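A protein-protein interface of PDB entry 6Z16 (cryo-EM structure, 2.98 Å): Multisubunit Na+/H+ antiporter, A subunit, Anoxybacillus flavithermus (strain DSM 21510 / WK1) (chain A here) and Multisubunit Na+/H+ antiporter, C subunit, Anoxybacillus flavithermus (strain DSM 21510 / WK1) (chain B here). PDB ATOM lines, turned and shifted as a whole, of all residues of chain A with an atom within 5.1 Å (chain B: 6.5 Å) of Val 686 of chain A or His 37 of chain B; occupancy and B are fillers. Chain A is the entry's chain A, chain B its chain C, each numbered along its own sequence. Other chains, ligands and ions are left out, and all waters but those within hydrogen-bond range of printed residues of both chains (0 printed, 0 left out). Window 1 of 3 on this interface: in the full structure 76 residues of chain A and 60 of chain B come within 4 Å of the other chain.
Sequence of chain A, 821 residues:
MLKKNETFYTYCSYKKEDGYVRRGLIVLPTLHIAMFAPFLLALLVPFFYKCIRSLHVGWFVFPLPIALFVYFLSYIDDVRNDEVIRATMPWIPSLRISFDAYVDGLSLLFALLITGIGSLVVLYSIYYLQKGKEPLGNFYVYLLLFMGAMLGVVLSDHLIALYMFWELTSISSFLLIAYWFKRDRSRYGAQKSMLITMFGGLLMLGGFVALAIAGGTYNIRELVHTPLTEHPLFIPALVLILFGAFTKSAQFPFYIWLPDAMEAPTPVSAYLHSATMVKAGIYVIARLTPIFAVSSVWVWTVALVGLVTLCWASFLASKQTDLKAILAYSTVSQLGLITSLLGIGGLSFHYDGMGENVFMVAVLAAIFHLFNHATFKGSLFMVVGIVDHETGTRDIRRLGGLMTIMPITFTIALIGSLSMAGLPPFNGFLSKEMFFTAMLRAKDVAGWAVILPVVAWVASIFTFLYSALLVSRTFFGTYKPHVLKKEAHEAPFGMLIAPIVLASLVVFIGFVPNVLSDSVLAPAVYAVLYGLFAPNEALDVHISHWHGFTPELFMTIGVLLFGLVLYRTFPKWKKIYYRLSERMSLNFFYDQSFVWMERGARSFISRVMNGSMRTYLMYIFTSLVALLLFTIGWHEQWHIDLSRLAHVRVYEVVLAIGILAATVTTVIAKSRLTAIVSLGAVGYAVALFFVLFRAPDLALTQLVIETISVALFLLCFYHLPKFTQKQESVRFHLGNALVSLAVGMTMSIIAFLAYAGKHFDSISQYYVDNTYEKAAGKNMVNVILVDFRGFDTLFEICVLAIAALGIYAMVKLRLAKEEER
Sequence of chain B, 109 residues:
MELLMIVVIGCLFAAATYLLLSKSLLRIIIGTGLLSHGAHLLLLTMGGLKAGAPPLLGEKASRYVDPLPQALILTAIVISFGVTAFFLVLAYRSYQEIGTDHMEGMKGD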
ATOM      1  N   LEU A 679     -26.412   3.140  22.670  1.00  0.00           N
ATOM      2  CA  LEU A 679     -26.986   4.327  23.297  1.00  0.00           C
ATOM      3  C   LEU A 679     -26.059   4.879  24.370  1.00  0.00           C
ATOM      4  O   LEU A 679     -25.932   6.102  24.527  1.00  0.00           O
ATOM      5  CB  LEU A 679     -28.356   3.990  23.883  1.00  0.00           C
ATOM      6  CG  LEU A 679     -29.106   5.108  24.601  1.00  0.00           C
ATOM      7  CD1 LEU A 679     -29.352   6.271  23.669  1.00  0.00           C
ATOM      8  CD2 LEU A 679     -30.409   4.576  25.136  1.00  0.00           C
ATOM      9  N   ALA A 681     -22.750   4.596  24.176  1.00  0.00           N
ATOM     10  CA  ALA A 681     -21.679   5.235  23.416  1.00  0.00           C
ATOM     11  C   ALA A 681     -22.109   6.590  22.868  1.00  0.00           C
ATOM     12  O   ALA A 681     -21.306   7.532  22.833  1.00  0.00           O
ATOM     13  CB  ALA A 681     -21.228   4.322  22.281  1.00  0.00           C
ATOM     14  N   VAL A 682     -23.378   6.708  22.458  1.00  0.00           N
ATOM     15  CA  VAL A 682     -23.950   8.001  22.079  1.00  0.00           C
ATOM     16  C   VAL A 682     -23.894   8.974  23.249  1.00  0.00           C
ATOM     17  O   VAL A 682     -23.509  10.134  23.079  1.00  0.00           O
ATOM     18  CB  VAL A 682     -25.392   7.827  21.558  1.00  0.00           C
ATOM     19  CG1 VAL A 682     -26.078   9.165  21.381  1.00  0.00           C
ATOM     20  CG2 VAL A 682     -25.396   7.133  20.229  1.00  0.00           C
ATOM     21  N   GLY A 683     -24.226   8.503  24.455  1.00  0.00           N
ATOM     22  CA  GLY A 683     -24.198   9.381  25.621  1.00  0.00           C
ATOM     23  C   GLY A 683     -22.804   9.871  25.978  1.00  0.00           C
ATOM     24  O   GLY A 683     -22.593  11.069  26.217  1.00  0.00           O
ATOM     25  N   TYR A 684     -21.827   8.959  25.984  1.00  0.00           N
ATOM     26  CA  TYR A 684     -20.460   9.360  26.316  1.00  0.00           C
ATOM     27  C   TYR A 684     -19.844  10.227  25.225  1.00  0.00           C
ATOM     28  O   TYR A 684     -19.047  11.124  25.516  1.00  0.00           O
ATOM     29  CB  TYR A 684     -19.579   8.141  26.594  1.00  0.00           C
ATOM     30  CG  TYR A 684     -19.964   7.391  27.849  1.00  0.00           C
ATOM     31  CD1 TYR A 684     -19.786   7.958  29.091  1.00  0.00           C
ATOM     32  CD2 TYR A 684     -20.443   6.093  27.795  1.00  0.00           C
ATOM     33  CE1 TYR A 684     -20.128   7.286  30.238  1.00  0.00           C
ATOM     34  CE2 TYR A 684     -20.795   5.410  28.936  1.00  0.00           C
ATOM     35  CZ  TYR A 684     -20.625   6.010  30.155  1.00  0.00           C
ATOM     36  OH  TYR A 684     -20.960   5.332  31.298  1.00  0.00           O
ATOM     37  N   ALA A 685     -20.253  10.041  23.975  1.00  0.00           N
ATOM     38  CA  ALA A 685     -19.729  10.910  22.936  1.00  0.00           C
ATOM     39  C   ALA A 685     -20.439  12.260  22.884  1.00  0.00           C
ATOM     40  O   ALA A 685     -19.837  13.245  22.447  1.00  0.00           O
ATOM     41  CB  ALA A 685     -19.815  10.201  21.601  1.00  0.00           C
ATOM     42  N   VAL A 686     -21.690  12.344  23.345  1.00  0.00           N
ATOM     43  CA  VAL A 686     -22.313  13.653  23.549  1.00  0.00           C
ATOM     44  C   VAL A 686     -21.598  14.401  24.668  1.00  0.00           C
ATOM     45  O   VAL A 686     -21.380  15.618  24.585  1.00  0.00           O
ATOM     46  CB  VAL A 686     -23.827  13.495  23.814  1.00  0.00           C
ATOM     47  CG1 VAL A 686     -24.449  14.776  24.331  1.00  0.00           C
ATOM     48  CG2 VAL A 686     -24.543  13.123  22.536  1.00  0.00           C
ATOM     49  N   ALA A 687     -21.166  13.670  25.702  1.00  0.00           N
ATOM     50  CA  ALA A 687     -20.312  14.263  26.733  1.00  0.00           C
ATOM     51  C   ALA A 687     -18.980  14.739  26.162  1.00  0.00           C
ATOM     52  O   ALA A 687     -18.455  15.780  26.575  1.00  0.00           O
ATOM     53  CB  ALA A 687     -20.079  13.260  27.857  1.00  0.00           C
ATOM     54  N   LEU A 688     -18.423  14.002  25.200  1.00  0.00           N
ATOM     55  CA  LEU A 688     -17.175  14.449  24.585  1.00  0.00           C
ATOM     56  C   LEU A 688     -17.390  15.662  23.679  1.00  0.00           C
ATOM     57  O   LEU A 688     -16.491  16.503  23.554  1.00  0.00           O
ATOM     58  CB  LEU A 688     -16.523  13.293  23.827  1.00  0.00           C
ATOM     59  CG  LEU A 688     -15.126  13.521  23.251  1.00  0.00           C
ATOM     60  CD1 LEU A 688     -14.152  13.902  24.349  1.00  0.00           C
ATOM     61  CD2 LEU A 688     -14.652  12.270  22.545  1.00  0.00           C
ATOM     62  N   PHE A 689     -18.568  15.779  23.057  1.00  0.00           N
ATOM     63  CA  PHE A 689     -18.935  17.032  22.392  1.00  0.00           C
ATOM     64  C   PHE A 689     -19.020  18.187  23.379  1.00  0.00           C
ATOM     65  O   PHE A 689     -18.608  19.311  23.067  1.00  0.00           O
ATOM     66  CB  PHE A 689     -20.276  16.921  21.666  1.00  0.00           C
ATOM     67  CG  PHE A 689     -20.205  16.286  20.314  1.00  0.00           C
ATOM     68  CD1 PHE A 689     -19.575  16.940  19.273  1.00  0.00           C
ATOM     69  CD2 PHE A 689     -20.855  15.095  20.053  1.00  0.00           C
ATOM     70  CE1 PHE A 689     -19.530  16.390  18.016  1.00  0.00           C
ATOM     71  CE2 PHE A 689     -20.821  14.540  18.797  1.00  0.00           C
ATOM     72  CZ  PHE A 689     -20.160  15.192  17.775  1.00  0.00           C
ATOM     73  N   PHE A 690     -19.593  17.933  24.558  1.00  0.00           N
ATOM     74  CA  PHE A 690     -19.706  18.966  25.586  1.00  0.00           C
ATOM     75  C   PHE A 690     -18.336  19.429  26.062  1.00  0.00           C
ATOM     76  O   PHE A 690     -18.139  20.618  26.332  1.00  0.00           O
ATOM     77  CB  PHE A 690     -20.530  18.441  26.757  1.00  0.00           C
ATOM     78  CG  PHE A 690     -22.003  18.357  26.481  1.00  0.00           C
ATOM     79  CD1 PHE A 690     -22.586  19.127  25.488  1.00  0.00           C
ATOM     80  CD2 PHE A 690     -22.802  17.492  27.210  1.00  0.00           C
ATOM     81  CE1 PHE A 690     -23.938  19.046  25.238  1.00  0.00           C
ATOM     82  CE2 PHE A 690     -24.151  17.405  26.962  1.00  0.00           C
ATOM     83  CZ  PHE A 690     -24.720  18.181  25.976  1.00  0.00           C
ATOM     84  N   GLN A 702     -23.380  14.938  32.363  1.00  0.00           N
ATOM     85  CA  GLN A 702     -23.731  14.032  31.281  1.00  0.00           C
ATOM     86  C   GLN A 702     -23.090  12.666  31.468  1.00  0.00           C
ATOM     87  O   GLN A 702     -23.753  11.644  31.273  1.00  0.00           O
ATOM     88  CB  GLN A 702     -23.304  14.647  29.949  1.00  0.00           C
ATOM     89  CG  GLN A 702     -23.723  13.863  28.725  1.00  0.00           C
ATOM     90  CD  GLN A 702     -25.199  13.979  28.444  1.00  0.00           C
ATOM     91  OE1 GLN A 702     -25.768  15.060  28.527  1.00  0.00           O
ATOM     92  NE2 GLN A 702     -25.829  12.867  28.109  1.00  0.00           N
ATOM     93  N   GLU A 706     -25.465   9.473  32.217  1.00  0.00           N
ATOM     94  CA  GLU A 706     -25.489   8.384  31.247  1.00  0.00           C
ATOM     95  C   GLU A 706     -25.034   7.066  31.845  1.00  0.00           C
ATOM     96  O   GLU A 706     -25.571   6.023  31.468  1.00  0.00           O
ATOM     97  CB  GLU A 706     -24.651   8.715  30.019  1.00  0.00           C
ATOM     98  CG  GLU A 706     -25.305   9.761  29.165  1.00  0.00           C
ATOM     99  CD  GLU A 706     -26.638   9.309  28.603  1.00  0.00           C
ATOM    100  OE1 GLU A 706     -26.757   8.133  28.196  1.00  0.00           O
ATOM    101  OE2 GLU A 706     -27.587  10.122  28.610  1.00  0.00           O
ATOM    102  N   ILE B   9     -27.766  16.027  14.197  1.00  0.00           N
ATOM    103  CA  ILE B   9     -28.958  15.974  15.046  1.00  0.00           C
ATOM    104  C   ILE B   9     -30.158  15.522  14.232  1.00  0.00           C
ATOM    105  O   ILE B   9     -31.103  14.943  14.782  1.00  0.00           O
ATOM    106  CB  ILE B   9     -29.234  17.310  15.779  1.00  0.00           C
ATOM    107  CG1 ILE B   9     -29.471  18.498  14.838  1.00  0.00           C
ATOM    108  CG2 ILE B   9     -28.119  17.631  16.740  1.00  0.00           C
ATOM    109  CD1 ILE B   9     -30.920  18.853  14.542  1.00  0.00           C
ATOM    110  N   LEU B  12     -29.960  11.846  14.499  1.00  0.00           N
ATOM    111  CA  LEU B  12     -30.467  11.449  15.813  1.00  0.00           C
ATOM    112  C   LEU B  12     -31.992  11.498  15.869  1.00  0.00           C
ATOM    113  O   LEU B  12     -32.624  10.606  16.445  1.00  0.00           O
ATOM    114  CB  LEU B  12     -29.862  12.328  16.905  1.00  0.00           C
ATOM    115  CG  LEU B  12     -28.404  12.030  17.233  1.00  0.00           C
ATOM    116  CD1 LEU B  12     -27.843  13.077  18.156  1.00  0.00           C
ATOM    117  CD2 LEU B  12     -28.314  10.672  17.874  1.00  0.00           C
ATOM    118  N   PHE B  13     -32.595  12.514  15.247  1.00  0.00           N
ATOM    119  CA  PHE B  13     -34.052  12.623  15.195  1.00  0.00           C
ATOM    120  C   PHE B  13     -34.677  11.514  14.363  1.00  0.00           C
ATOM    121  O   PHE B  13     -35.696  10.939  14.759  1.00  0.00           O
ATOM    122  CB  PHE B  13     -34.443  13.986  14.640  1.00  0.00           C
ATOM    123  CG  PHE B  13     -34.309  15.098  15.629  1.00  0.00           C
ATOM    124  CD1 PHE B  13     -34.385  14.844  16.985  1.00  0.00           C
ATOM    125  CD2 PHE B  13     -34.066  16.390  15.205  1.00  0.00           C
ATOM    126  CE1 PHE B  13     -34.261  15.860  17.897  1.00  0.00           C
ATOM    127  CE2 PHE B  13     -33.934  17.412  16.114  1.00  0.00           C
ATOM    128  CZ  PHE B  13     -34.030  17.146  17.462  1.00  0.00           C
ATOM    129  N   THR B  32     -36.443   7.221  22.980  1.00  0.00           N
ATOM    130  CA  THR B  32     -36.609   8.353  23.891  1.00  0.00           C
ATOM    131  C   THR B  32     -35.264   8.963  24.275  1.00  0.00           C
ATOM    132  O   THR B  32     -35.089  10.192  24.237  1.00  0.00           O
ATOM    133  CB  THR B  32     -37.374   7.891  25.134  1.00  0.00           C
ATOM    134  OG1 THR B  32     -38.754   7.678  24.810  1.00  0.00           O
ATOM    135  CG2 THR B  32     -37.225   8.858  26.290  1.00  0.00           C
ATOM    136  N   GLY B  33     -34.295   8.105  24.615  1.00  0.00           N
ATOM    137  CA  GLY B  33     -32.954   8.583  24.934  1.00  0.00           C
ATOM    138  C   GLY B  33     -32.281   9.306  23.780  1.00  0.00           C
ATOM    139  O   GLY B  33     -31.710  10.389  23.963  1.00  0.00           O
ATOM    140  N   LEU B  34     -32.373   8.740  22.571  1.00  0.00           N
ATOM    141  CA  LEU B  34     -31.780   9.385  21.399  1.00  0.00           C
ATOM    142  C   LEU B  34     -32.458  10.707  21.061  1.00  0.00           C
ATOM    143  O   LEU B  34     -31.785  11.652  20.626  1.00  0.00           O
ATOM    144  CB  LEU B  34     -31.836   8.449  20.195  1.00  0.00           C
ATOM    145  CG  LEU B  34     -30.934   7.223  20.245  1.00  0.00           C
ATOM    146  CD1 LEU B  34     -31.238   6.333  19.083  1.00  0.00           C
ATOM    147  CD2 LEU B  34     -29.491   7.647  20.201  1.00  0.00           C
ATOM    148  N   LEU B  35     -33.773  10.800  21.276  1.00  0.00           N
ATOM    149  CA  LEU B  35     -34.489  12.050  21.035  1.00  0.00           C
ATOM    150  C   LEU B  35     -34.068  13.124  22.027  1.00  0.00           C
ATOM    151  O   LEU B  35     -33.944  14.303  21.665  1.00  0.00           O
ATOM    152  CB  LEU B  35     -35.994  11.795  21.116  1.00  0.00           C
ATOM    153  CG  LEU B  35     -36.969  12.915  20.778  1.00  0.00           C
ATOM    154  CD1 LEU B  35     -36.809  13.340  19.342  1.00  0.00           C
ATOM    155  CD2 LEU B  35     -38.377  12.437  21.032  1.00  0.00           C
ATOM    156  N   SER B  36     -33.816  12.722  23.277  1.00  0.00           N
ATOM    157  CA  SER B  36     -33.313  13.658  24.278  1.00  0.00           C
ATOM    158  C   SER B  36     -31.923  14.173  23.919  1.00  0.00           C
ATOM    159  O   SER B  36     -31.651  15.375  24.049  1.00  0.00           O
ATOM    160  CB  SER B  36     -33.291  12.989  25.648  1.00  0.00           C
ATOM    161  OG  SER B  36     -34.597  12.629  26.048  1.00  0.00           O
ATOM    162  N   HIS B  37     -31.033  13.274  23.472  1.00  0.00           N
ATOM    163  CA  HIS B  37     -29.696  13.694  23.046  1.00  0.00           C
ATOM    164  C   HIS B  37     -29.757  14.654  21.867  1.00  0.00           C
ATOM    165  O   HIS B  37     -29.013  15.645  21.825  1.00  0.00           O
ATOM    166  CB  HIS B  37     -28.831  12.494  22.673  1.00  0.00           C
ATOM    167  CG  HIS B  37     -28.428  11.645  23.835  1.00  0.00           C
ATOM    168  ND1 HIS B  37     -27.582  12.097  24.821  1.00  0.00           N
ATOM    169  CD2 HIS B  37     -28.686  10.350  24.127  1.00  0.00           C
ATOM    170  CE1 HIS B  37     -27.380  11.133  25.698  1.00  0.00           C
ATOM    171  NE2 HIS B  37     -28.039  10.061  25.300  1.00  0.00           N
ATOM    172  N   GLY B  38     -30.652  14.383  20.913  1.00  0.00           N
ATOM    173  CA  GLY B  38     -30.805  15.277  19.779  1.00  0.00           C
ATOM    174  C   GLY B  38     -31.313  16.649  20.173  1.00  0.00           C
ATOM    175  O   GLY B  38     -30.825  17.665  19.672  1.00  0.00           O
ATOM    176  N   ALA B  39     -32.258  16.699  21.120  1.00  0.00           N
ATOM    177  CA  ALA B  39     -32.790  17.986  21.569  1.00  0.00           C
ATOM    178  C   ALA B  39     -31.743  18.800  22.321  1.00  0.00           C
ATOM    179  O   ALA B  39     -31.652  20.024  22.144  1.00  0.00           O
ATOM    180  CB  ALA B  39     -34.022  17.763  22.441  1.00  0.00           C
ATOM    181  N   HIS B  40     -30.918  18.134  23.135  1.00  0.00           N
ATOM    182  CA  HIS B  40     -29.922  18.856  23.922  1.00  0.00           C
ATOM    183  C   HIS B  40     -28.788  19.371  23.041  1.00  0.00           C
ATOM    184  O   HIS B  40     -28.336  20.518  23.200  1.00  0.00           O
ATOM    185  CB  HIS B  40     -29.385  17.949  25.023  1.00  0.00           C
ATOM    186  CG  HIS B  40     -30.438  17.463  25.968  1.00  0.00           C
ATOM    187  ND1 HIS B  40     -30.227  16.422  26.843  1.00  0.00           N
ATOM    188  CD2 HIS B  40     -31.716  17.864  26.162  1.00  0.00           C
ATOM    189  CE1 HIS B  40     -31.329  16.199  27.534  1.00  0.00           C
ATOM    190  NE2 HIS B  40     -32.248  17.061  27.139  1.00  0.00           N
ATOM    191  N   LEU B  41     -28.337  18.547  22.085  1.00  0.00           N
ATOM    192  CA  LEU B  41     -27.362  19.014  21.107  1.00  0.00           C
ATOM    193  C   LEU B  41     -27.922  20.127  20.238  1.00  0.00           C
ATOM    194  O   LEU B  41     -27.177  21.021  19.827  1.00  0.00           O
ATOM    195  CB  LEU B  41     -26.891  17.857  20.230  1.00  0.00           C
ATOM    196  CG  LEU B  41     -25.971  16.818  20.856  1.00  0.00           C
ATOM    197  CD1 LEU B  41     -25.776  15.668  19.907  1.00  0.00           C
ATOM    198  CD2 LEU B  41     -24.641  17.459  21.174  1.00  0.00           C
ATOM    199  N   LEU B  42     -29.232  20.114  19.977  1.00  0.00           N
ATOM    200  CA  LEU B  42     -29.828  21.186  19.194  1.00  0.00           C
ATOM    201  C   LEU B  42     -29.866  22.493  19.973  1.00  0.00           C
ATOM    202  O   LEU B  42     -29.638  23.560  19.397  1.00  0.00           O
ATOM    203  CB  LEU B  42     -31.225  20.784  18.734  1.00  0.00           C
ATOM    204  CG  LEU B  42     -31.921  21.781  17.814  1.00  0.00           C
ATOM    205  CD1 LEU B  42     -31.111  21.991  16.564  1.00  0.00           C
ATOM    206  CD2 LEU B  42     -33.279  21.269  17.457  1.00  0.00           C
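Leu 679 of chain A touches Leu 34 of chain B (CD1 to CD2, 3.7 Å).
CG1 of Val 682 of chain A touches CD2 of Leu 34 of chain B, 3.9 Å away.
His 37 of chain B touches Val 682 of chain A (CD2 to CG1, 3.97 Å).
Gly 683 of chain A touches His 37 of chain B.
Val 686 of chain A touches His 37 of chain B.
Leu 41 of chain B touches Val 686 of chain A (CD1 to CG2, 3.9 Å).
Gln 702 of chain A touches His 37 of chain B (NE2 to CE1, 3.4 Å).
OE2 of Glu 706 of chain A lies close to NE2 of His 37 of chain B, 3.3 Å away.
The side-chain amide nitrogen (NE2) of Gln 702 of chain A lies within hydrogen-bond range of the side-chain carboxylate (OE2) of Glu 706 of chain A (3.3 Å).
Of the printed residues of chain B, Leu 679 of chain A touches Leu 34.
Of the printed residues of chain B, Gly 683 of chain A touches His 37.
Leu 688 of chain A touches none of the printed residues of chain B.
Of the printed residues of chain B, Glu 706 of chain A touches His 37 (3.1 Å).
Ile 9 of chain B touches none of the printed residues of chain A.
Of the printed residues of chain A, Leu 34 of chain B touches Leu 679 (3.7 Å) and Val 682 (3.9 Å).
His 37 of chain B touches five residues of chain A.
Printed residues of chain A within 4 Å of Leu 41 of chain B: Val 686.
The nearest printed residue of chain A that does not touch Leu 41 of chain B is Phe 690 of chain A (4.4 Å).
Hydrophobic or aromatic side chains of chain B that line the printed part of chain A: Leu 34, His 37 and Leu 41.
Of the 13 printed residues of chain A, 6 touch a printed residue of chain B.
Printed residues of chain A that touch a printed residue of chain B: Leu 679, Val 682, Gly 683, Val 686, Gln 702 and Glu 706.
Hydrophobic or aromatic side chains of chain A within 4 Å of the printed part of chain B: Leu 679, Val 682 and Val 686.
Among the printed residues, no Asp or Glu carboxylate lies within 4 Å of a Lys or Arg side-chain nitrogen of the other chain.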
